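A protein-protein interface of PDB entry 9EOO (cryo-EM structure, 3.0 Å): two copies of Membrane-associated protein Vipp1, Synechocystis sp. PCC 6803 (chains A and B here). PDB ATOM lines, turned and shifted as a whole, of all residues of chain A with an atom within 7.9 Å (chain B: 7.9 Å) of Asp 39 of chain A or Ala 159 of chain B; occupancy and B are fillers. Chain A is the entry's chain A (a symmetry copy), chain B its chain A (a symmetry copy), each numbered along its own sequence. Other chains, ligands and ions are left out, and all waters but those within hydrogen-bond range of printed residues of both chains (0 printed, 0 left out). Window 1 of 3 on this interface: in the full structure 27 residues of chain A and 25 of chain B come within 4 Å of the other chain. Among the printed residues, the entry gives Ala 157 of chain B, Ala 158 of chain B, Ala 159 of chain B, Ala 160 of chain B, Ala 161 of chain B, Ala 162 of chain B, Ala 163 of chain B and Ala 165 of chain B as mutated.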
ATOM      1  N   ALA A  32      16.372 -12.082  14.585  1.00  0.00           N
ATOM      2  CA  ALA A  32      16.235 -10.875  13.780  1.00  0.00           C
ATOM      3  C   ALA A  32      16.308  -9.605  14.615  1.00  0.00           C
ATOM      4  O   ALA A  32      16.848  -8.590  14.167  1.00  0.00           O
ATOM      5  CB  ALA A  32      14.921 -10.920  13.015  1.00  0.00           C
ATOM      6  N   VAL A  33      15.767  -9.637  15.827  1.00  0.00           N
ATOM      7  CA  VAL A  33      15.855  -8.483  16.714  1.00  0.00           C
ATOM      8  C   VAL A  33      17.240  -8.329  17.323  1.00  0.00           C
ATOM      9  O   VAL A  33      17.712  -7.207  17.529  1.00  0.00           O
ATOM     10  CB  VAL A  33      14.782  -8.603  17.805  1.00  0.00           C
ATOM     11  CG1 VAL A  33      14.821  -7.412  18.709  1.00  0.00           C
ATOM     12  CG2 VAL A  33      13.432  -8.738  17.183  1.00  0.00           C
ATOM     13  N   ILE A  34      17.913  -9.434  17.625  1.00  0.00           N
ATOM     14  CA  ILE A  34      19.305  -9.359  18.054  1.00  0.00           C
ATOM     15  C   ILE A  34      20.181  -8.712  16.992  1.00  0.00           C
ATOM     16  O   ILE A  34      20.949  -7.786  17.276  1.00  0.00           O
ATOM     17  CB  ILE A  34      19.814 -10.761  18.415  1.00  0.00           C
ATOM     18  CG1 ILE A  34      19.122 -11.258  19.676  1.00  0.00           C
ATOM     19  CG2 ILE A  34      21.302 -10.768  18.589  1.00  0.00           C
ATOM     20  CD1 ILE A  34      19.327 -12.700  19.922  1.00  0.00           C
ATOM     21  N   ASP A  35      20.085  -9.185  15.755  1.00  0.00           N
ATOM     22  CA  ASP A  35      20.876  -8.611  14.673  1.00  0.00           C
ATOM     23  C   ASP A  35      20.616  -7.121  14.508  1.00  0.00           C
ATOM     24  O   ASP A  35      21.548  -6.320  14.380  1.00  0.00           O
ATOM     25  CB  ASP A  35      20.567  -9.350  13.377  1.00  0.00           C
ATOM     26  CG  ASP A  35      21.037 -10.785  13.402  1.00  0.00           C
ATOM     27  OD1 ASP A  35      21.714 -11.171  14.378  1.00  0.00           O
ATOM     28  OD2 ASP A  35      20.735 -11.529  12.447  1.00  0.00           O
ATOM     29  N   MET A  36      19.349  -6.735  14.507  1.00  0.00           N
ATOM     30  CA  MET A  36      18.961  -5.339  14.372  1.00  0.00           C
ATOM     31  C   MET A  36      19.400  -4.467  15.543  1.00  0.00           C
ATOM     32  O   MET A  36      19.544  -3.252  15.379  1.00  0.00           O
ATOM     33  CB  MET A  36      17.456  -5.266  14.157  1.00  0.00           C
ATOM     34  CG  MET A  36      16.879  -3.897  14.267  1.00  0.00           C
ATOM     35  SD  MET A  36      15.293  -3.769  13.422  1.00  0.00           S
ATOM     36  CE  MET A  36      14.436  -5.183  14.087  1.00  0.00           C
ATOM     37  N   GLN A  37      19.608  -5.043  16.723  1.00  0.00           N
ATOM     38  CA  GLN A  37      20.145  -4.266  17.839  1.00  0.00           C
ATOM     39  C   GLN A  37      21.640  -3.987  17.725  1.00  0.00           C
ATOM     40  O   GLN A  37      22.082  -2.858  17.954  1.00  0.00           O
ATOM     41  CB  GLN A  37      19.862  -4.986  19.150  1.00  0.00           C
ATOM     42  CG  GLN A  37      18.470  -4.755  19.679  1.00  0.00           C
ATOM     43  CD  GLN A  37      18.231  -5.393  21.028  1.00  0.00           C
ATOM     44  OE1 GLN A  37      17.516  -4.845  21.863  1.00  0.00           O
ATOM     45  NE2 GLN A  37      18.822  -6.554  21.247  1.00  0.00           N
ATOM     46  N   GLU A  38      22.440  -4.992  17.378  1.00  0.00           N
ATOM     47  CA  GLU A  38      23.879  -4.771  17.263  1.00  0.00           C
ATOM     48  C   GLU A  38      24.256  -3.942  16.043  1.00  0.00           C
ATOM     49  O   GLU A  38      25.298  -3.282  16.043  1.00  0.00           O
ATOM     50  CB  GLU A  38      24.592  -6.111  17.214  1.00  0.00           C
ATOM     51  CG  GLU A  38      24.275  -6.905  15.985  1.00  0.00           C
ATOM     52  CD  GLU A  38      24.960  -8.252  15.977  1.00  0.00           C
ATOM     53  OE1 GLU A  38      25.718  -8.534  16.929  1.00  0.00           O
ATOM     54  OE2 GLU A  38      24.742  -9.031  15.026  1.00  0.00           O
ATOM     55  N   ASP A  39      23.434  -3.969  15.001  1.00  0.00           N
ATOM     56  CA  ASP A  39      23.585  -3.031  13.894  1.00  0.00           C
ATOM     57  C   ASP A  39      23.585  -1.582  14.363  1.00  0.00           C
ATOM     58  O   ASP A  39      24.343  -0.754  13.849  1.00  0.00           O
ATOM     59  CB  ASP A  39      22.471  -3.255  12.882  1.00  0.00           C
ATOM     60  CG  ASP A  39      22.518  -2.268  11.740  1.00  0.00           C
ATOM     61  OD1 ASP A  39      23.615  -1.751  11.441  1.00  0.00           O
ATOM     62  OD2 ASP A  39      21.455  -2.001  11.141  1.00  0.00           O
ATOM     63  N   LEU A  40      22.740  -1.259  15.334  1.00  0.00           N
ATOM     64  CA  LEU A  40      22.736   0.072  15.927  1.00  0.00           C
ATOM     65  C   LEU A  40      23.979   0.370  16.752  1.00  0.00           C
ATOM     66  O   LEU A  40      24.410   1.525  16.815  1.00  0.00           O
ATOM     67  CB  LEU A  40      21.503   0.215  16.809  1.00  0.00           C
ATOM     68  CG  LEU A  40      21.370   1.486  17.627  1.00  0.00           C
ATOM     69  CD1 LEU A  40      21.320   2.681  16.738  1.00  0.00           C
ATOM     70  CD2 LEU A  40      20.136   1.416  18.471  1.00  0.00           C
ATOM     71  N   VAL A  41      24.566  -0.634  17.392  1.00  0.00           N
ATOM     72  CA  VAL A  41      25.825  -0.423  18.099  1.00  0.00           C
ATOM     73  C   VAL A  41      26.962  -0.089  17.143  1.00  0.00           C
ATOM     74  O   VAL A  41      27.770   0.806  17.413  1.00  0.00           O
ATOM     75  CB  VAL A  41      26.150  -1.667  18.935  1.00  0.00           C
ATOM     76  CG1 VAL A  41      27.477  -1.521  19.613  1.00  0.00           C
ATOM     77  CG2 VAL A  41      25.080  -1.885  19.953  1.00  0.00           C
ATOM     78  N   GLN A  42      27.043  -0.788  16.016  1.00  0.00           N
ATOM     79  CA  GLN A  42      28.029  -0.449  14.997  1.00  0.00           C
ATOM     80  C   GLN A  42      27.788   0.929  14.399  1.00  0.00           C
ATOM     81  O   GLN A  42      28.732   1.697  14.193  1.00  0.00           O
ATOM     82  CB  GLN A  42      28.013  -1.504  13.902  1.00  0.00           C
ATOM     83  CG  GLN A  42      28.396  -2.880  14.376  1.00  0.00           C
ATOM     84  CD  GLN A  42      29.740  -2.907  15.061  1.00  0.00           C
ATOM     85  OE1 GLN A  42      30.672  -2.221  14.649  1.00  0.00           O
ATOM     86  NE2 GLN A  42      29.847  -3.700  16.115  1.00  0.00           N
ATOM     87  N   LEU A  43      26.536   1.256  14.115  1.00  0.00           N
ATOM     88  CA  LEU A  43      26.222   2.539  13.503  1.00  0.00           C
ATOM     89  C   LEU A  43      26.578   3.714  14.400  1.00  0.00           C
ATOM     90  O   LEU A  43      27.098   4.729  13.926  1.00  0.00           O
ATOM     91  CB  LEU A  43      24.738   2.582  13.164  1.00  0.00           C
ATOM     92  CG  LEU A  43      24.259   3.830  12.446  1.00  0.00           C
ATOM     93  CD1 LEU A  43      24.858   3.876  11.077  1.00  0.00           C
ATOM     94  CD2 LEU A  43      22.764   3.853  12.364  1.00  0.00           C
ATOM     95  N   ARG A  44      26.308   3.599  15.692  1.00  0.00           N
ATOM     96  CA  ARG A  44      26.558   4.705  16.607  1.00  0.00           C
ATOM     97  C   ARG A  44      28.043   5.023  16.736  1.00  0.00           C
ATOM     98  O   ARG A  44      28.422   6.190  16.882  1.00  0.00           O
ATOM     99  CB  ARG A  44      25.952   4.376  17.966  1.00  0.00           C
ATOM    100  CG  ARG A  44      25.903   5.542  18.908  1.00  0.00           C
ATOM    101  CD  ARG A  44      25.354   5.168  20.268  1.00  0.00           C
ATOM    102  NE  ARG A  44      23.943   4.812  20.228  1.00  0.00           N
ATOM    103  CZ  ARG A  44      23.434   3.657  20.635  1.00  0.00           C
ATOM    104  NH1 ARG A  44      24.204   2.649  21.009  1.00  0.00           N
ATOM    105  NH2 ARG A  44      22.115   3.506  20.662  1.00  0.00           N
ATOM    106  N   GLN A  45      28.899   4.007  16.682  1.00  0.00           N
ATOM    107  CA  GLN A  45      30.341   4.225  16.670  1.00  0.00           C
ATOM    108  C   GLN A  45      30.810   5.003  15.448  1.00  0.00           C
ATOM    109  O   GLN A  45      31.603   5.942  15.563  1.00  0.00           O
ATOM    110  CB  GLN A  45      31.055   2.883  16.706  1.00  0.00           C
ATOM    111  CG  GLN A  45      30.878   2.117  17.974  1.00  0.00           C
ATOM    112  CD  GLN A  45      31.601   0.793  17.938  1.00  0.00           C
ATOM    113  OE1 GLN A  45      32.527   0.603  17.153  1.00  0.00           O
ATOM    114  NE2 GLN A  45      31.183  -0.132  18.789  1.00  0.00           N
ATOM    115  N   LEU A 122      19.351   7.834  13.183  1.00  0.00           N
ATOM    116  CA  LEU A 122      19.714   6.978  14.302  1.00  0.00           C
ATOM    117  C   LEU A 122      18.586   6.820  15.315  1.00  0.00           C
ATOM    118  O   LEU A 122      18.420   5.744  15.898  1.00  0.00           O
ATOM    119  CB  LEU A 122      20.955   7.554  14.966  1.00  0.00           C
ATOM    120  CG  LEU A 122      21.668   6.731  16.016  1.00  0.00           C
ATOM    121  CD1 LEU A 122      22.312   5.556  15.367  1.00  0.00           C
ATOM    122  CD2 LEU A 122      22.710   7.582  16.664  1.00  0.00           C
ATOM    123  N   LEU A 125      15.626   4.548  13.940  1.00  0.00           N
ATOM    124  CA  LEU A 125      15.899   3.118  14.025  1.00  0.00           C
ATOM    125  C   LEU A 125      15.486   2.520  15.364  1.00  0.00           C
ATOM    126  O   LEU A 125      14.738   1.541  15.408  1.00  0.00           O
ATOM    127  CB  LEU A 125      17.381   2.882  13.773  1.00  0.00           C
ATOM    128  CG  LEU A 125      17.895   1.458  13.903  1.00  0.00           C
ATOM    129  CD1 LEU A 125      17.101   0.508  13.058  1.00  0.00           C
ATOM    130  CD2 LEU A 125      19.344   1.418  13.513  1.00  0.00           C
ATOM    131  N   ILE A 129      12.927  -0.655  16.586  1.00  0.00           N
ATOM    132  CA  ILE A 129      13.336  -1.810  17.378  1.00  0.00           C
ATOM    133  C   ILE A 129      12.392  -2.021  18.551  1.00  0.00           C
ATOM    134  O   ILE A 129      11.995  -3.152  18.853  1.00  0.00           O
ATOM    135  CB  ILE A 129      14.783  -1.644  17.864  1.00  0.00           C
ATOM    136  CG1 ILE A 129      15.709  -1.382  16.685  1.00  0.00           C
ATOM    137  CG2 ILE A 129      15.225  -2.859  18.634  1.00  0.00           C
ATOM    138  CD1 ILE A 129      17.151  -1.345  17.055  1.00  0.00           C
ATOM    139  N   GLN B 153      29.535   4.422   5.458  1.00  0.00           N
ATOM    140  CA  GLN B 153      28.722   4.001   4.326  1.00  0.00           C
ATOM    141  C   GLN B 153      28.816   2.504   4.072  1.00  0.00           C
ATOM    142  O   GLN B 153      27.868   1.904   3.558  1.00  0.00           O
ATOM    143  CB  GLN B 153      29.146   4.770   3.082  1.00  0.00           C
ATOM    144  CG  GLN B 153      28.836   6.250   3.140  1.00  0.00           C
ATOM    145  CD  GLN B 153      27.356   6.539   3.236  1.00  0.00           C
ATOM    146  OE1 GLN B 153      26.526   5.733   2.820  1.00  0.00           O
ATOM    147  NE2 GLN B 153      27.018   7.695   3.795  1.00  0.00           N
ATOM    148  N   GLN B 154      29.939   1.888   4.423  1.00  0.00           N
ATOM    149  CA  GLN B 154      30.048   0.437   4.358  1.00  0.00           C
ATOM    150  C   GLN B 154      29.207  -0.261   5.418  1.00  0.00           C
ATOM    151  O   GLN B 154      28.702  -1.363   5.181  1.00  0.00           O
ATOM    152  CB  GLN B 154      31.508   0.042   4.509  1.00  0.00           C
ATOM    153  CG  GLN B 154      31.766  -1.428   4.438  1.00  0.00           C
ATOM    154  CD  GLN B 154      33.242  -1.744   4.482  1.00  0.00           C
ATOM    155  OE1 GLN B 154      34.070  -0.860   4.691  1.00  0.00           O
ATOM    156  NE2 GLN B 154      33.583  -3.009   4.284  1.00  0.00           N
ATOM    157  N   THR B 155      29.060   0.353   6.587  1.00  0.00           N
ATOM    158  CA  THR B 155      28.249  -0.227   7.649  1.00  0.00           C
ATOM    159  C   THR B 155      26.763  -0.215   7.310  1.00  0.00           C
ATOM    160  O   THR B 155      26.059  -1.204   7.540  1.00  0.00           O
ATOM    161  CB  THR B 155      28.507   0.528   8.949  1.00  0.00           C
ATOM    162  OG1 THR B 155      29.881   0.379   9.319  1.00  0.00           O
ATOM    163  CG2 THR B 155      27.646   0.006  10.057  1.00  0.00           C
ATOM    164  N   LEU B 156      26.271   0.894   6.768  1.00  0.00           N
ATOM    165  CA  LEU B 156      24.878   0.991   6.348  1.00  0.00           C
ATOM    166  C   LEU B 156      24.521   0.026   5.228  1.00  0.00           C
ATOM    167  O   LEU B 156      23.385  -0.452   5.165  1.00  0.00           O
ATOM    168  CB  LEU B 156      24.589   2.413   5.896  1.00  0.00           C
ATOM    169  CG  LEU B 156      24.139   3.375   6.981  1.00  0.00           C
ATOM    170  CD1 LEU B 156      25.172   3.415   8.034  1.00  0.00           C
ATOM    171  CD2 LEU B 156      23.944   4.752   6.428  1.00  0.00           C
ATOM    172  N   ALA B 157      25.461  -0.270   4.340  1.00  0.00           N
ATOM    173  CA  ALA B 157      25.201  -1.244   3.287  1.00  0.00           C
ATOM    174  C   ALA B 157      25.047  -2.660   3.832  1.00  0.00           C
ATOM    175  O   ALA B 157      24.107  -3.374   3.467  1.00  0.00           O
ATOM    176  CB  ALA B 157      26.327  -1.195   2.266  1.00  0.00           C
ATOM    177  N   ALA B 158      25.954  -3.084   4.705  1.00  0.00           N
ATOM    178  CA  ALA B 158      25.866  -4.426   5.270  1.00  0.00           C
ATOM    179  C   ALA B 158      24.605  -4.620   6.107  1.00  0.00           C
ATOM    180  O   ALA B 158      24.020  -5.709   6.112  1.00  0.00           O
ATOM    181  CB  ALA B 158      27.104  -4.714   6.110  1.00  0.00           C
ATOM    182  N   ALA B 159      24.171  -3.584   6.824  1.00  0.00           N
ATOM    183  CA  ALA B 159      22.911  -3.659   7.551  1.00  0.00           C
ATOM    184  C   ALA B 159      21.728  -3.863   6.616  1.00  0.00           C
ATOM    185  O   ALA B 159      20.869  -4.719   6.856  1.00  0.00           O
ATOM    186  CB  ALA B 159      22.718  -2.392   8.380  1.00  0.00           C
ATOM    187  N   ALA B 160      21.667  -3.082   5.542  1.00  0.00           N
ATOM    188  CA  ALA B 160      20.604  -3.234   4.557  1.00  0.00           C
ATOM    189  C   ALA B 160      20.685  -4.560   3.816  1.00  0.00           C
ATOM    190  O   ALA B 160      19.666  -5.054   3.324  1.00  0.00           O
ATOM    191  CB  ALA B 160      20.651  -2.077   3.565  1.00  0.00           C
ATOM    192  N   ALA B 161      21.873  -5.147   3.726  1.00  0.00           N
ATOM    193  CA  ALA B 161      22.013  -6.461   3.113  1.00  0.00           C
ATOM    194  C   ALA B 161      21.538  -7.592   4.014  1.00  0.00           C
ATOM    195  O   ALA B 161      21.078  -8.621   3.508  1.00  0.00           O
ATOM    196  CB  ALA B 161      23.469  -6.701   2.725  1.00  0.00           C
ATOM    197  N   ALA B 162      21.639  -7.440   5.334  1.00  0.00           N
ATOM    198  CA  ALA B 162      21.088  -8.456   6.224  1.00  0.00           C
ATOM    199  C   ALA B 162      19.564  -8.410   6.260  1.00  0.00           C
ATOM    200  O   ALA B 162      18.911  -9.460   6.302  1.00  0.00           O
ATOM    201  CB  ALA B 162      21.660  -8.279   7.627  1.00  0.00           C
ATOM    202  N   ALA B 163      18.980  -7.216   6.235  1.00  0.00           N
ATOM    203  CA  ALA B 163      17.532  -7.055   6.110  1.00  0.00           C
ATOM    204  C   ALA B 163      16.797  -7.918   7.131  1.00  0.00           C
ATOM    205  O   ALA B 163      15.887  -8.684   6.807  1.00  0.00           O
ATOM    206  CB  ALA B 163      17.077  -7.379   4.694  1.00  0.00           C
ATOM    207  N   ALA B 164      17.215  -7.788   8.387  1.00  0.00           N
ATOM    208  CA  ALA B 164      16.570  -8.496   9.483  1.00  0.00           C
ATOM    209  C   ALA B 164      15.103  -8.122   9.632  1.00  0.00           C
ATOM    210  O   ALA B 164      14.287  -8.955  10.039  1.00  0.00           O
ATOM    211  CB  ALA B 164      17.316  -8.213  10.778  1.00  0.00           C
ATOM    212  N   ALA B 165      14.748  -6.882   9.306  1.00  0.00           N
ATOM    213  CA  ALA B 165      13.365  -6.437   9.399  1.00  0.00           C
ATOM    214  C   ALA B 165      12.471  -7.038   8.326  1.00  0.00           C
ATOM    215  O   ALA B 165      11.246  -7.031   8.486  1.00  0.00           O
ATOM    216  CB  ALA B 165      13.301  -4.920   9.311  1.00  0.00           C
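Met 36 of chain A touches none of the printed residues of chain B. Printed residues of chain B within 4 Å of Leu 43 of chain A: Leu 156 (3.1 Å). Arg 44 of chain A touches none of the printed residues of chain B. Of the printed residues of chain A, Leu 156 of chain B touches Leu 43 (3.1 Å). No residue of chain A comes within 4 Å of Ala 158 of chain B. Ala 159 of chain B touches just one residue of chain A: Asp 39 (3.1 Å). Printed residues of chain A within 4 Å of Ala 164 of chain B: Ala 32 (3.4 Å).
Printed residues of chain A that touch a printed residue of chain B: Ala 32, Asp 39 and Leu 43. Hydrophobic or aromatic side chains of chain A within 4 Å of the printed part of chain B: Ala 32 and Leu 43. Along chain A the printed residues that touch a printed residue of chain B span positions 32 to 43. Printed residues of chain B that touch a printed residue of chain A: Leu 156, Ala 159 and Ala 164. Among the printed residues, 3 pairs touch across the chains. Among the printed residues, no Asp or Glu carboxylate lies within 4 Å of a Lys or Arg side-chain nitrogen of the other chain.
Among the printed residues, merely in contact across the chains: Ala 32 of chain A with Ala 164 of chain B, Asp 39 of chain A with Ala 159 of chain B and Leu 43 of chain A with Leu 156 of chain B.
No position is printed for both chains.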
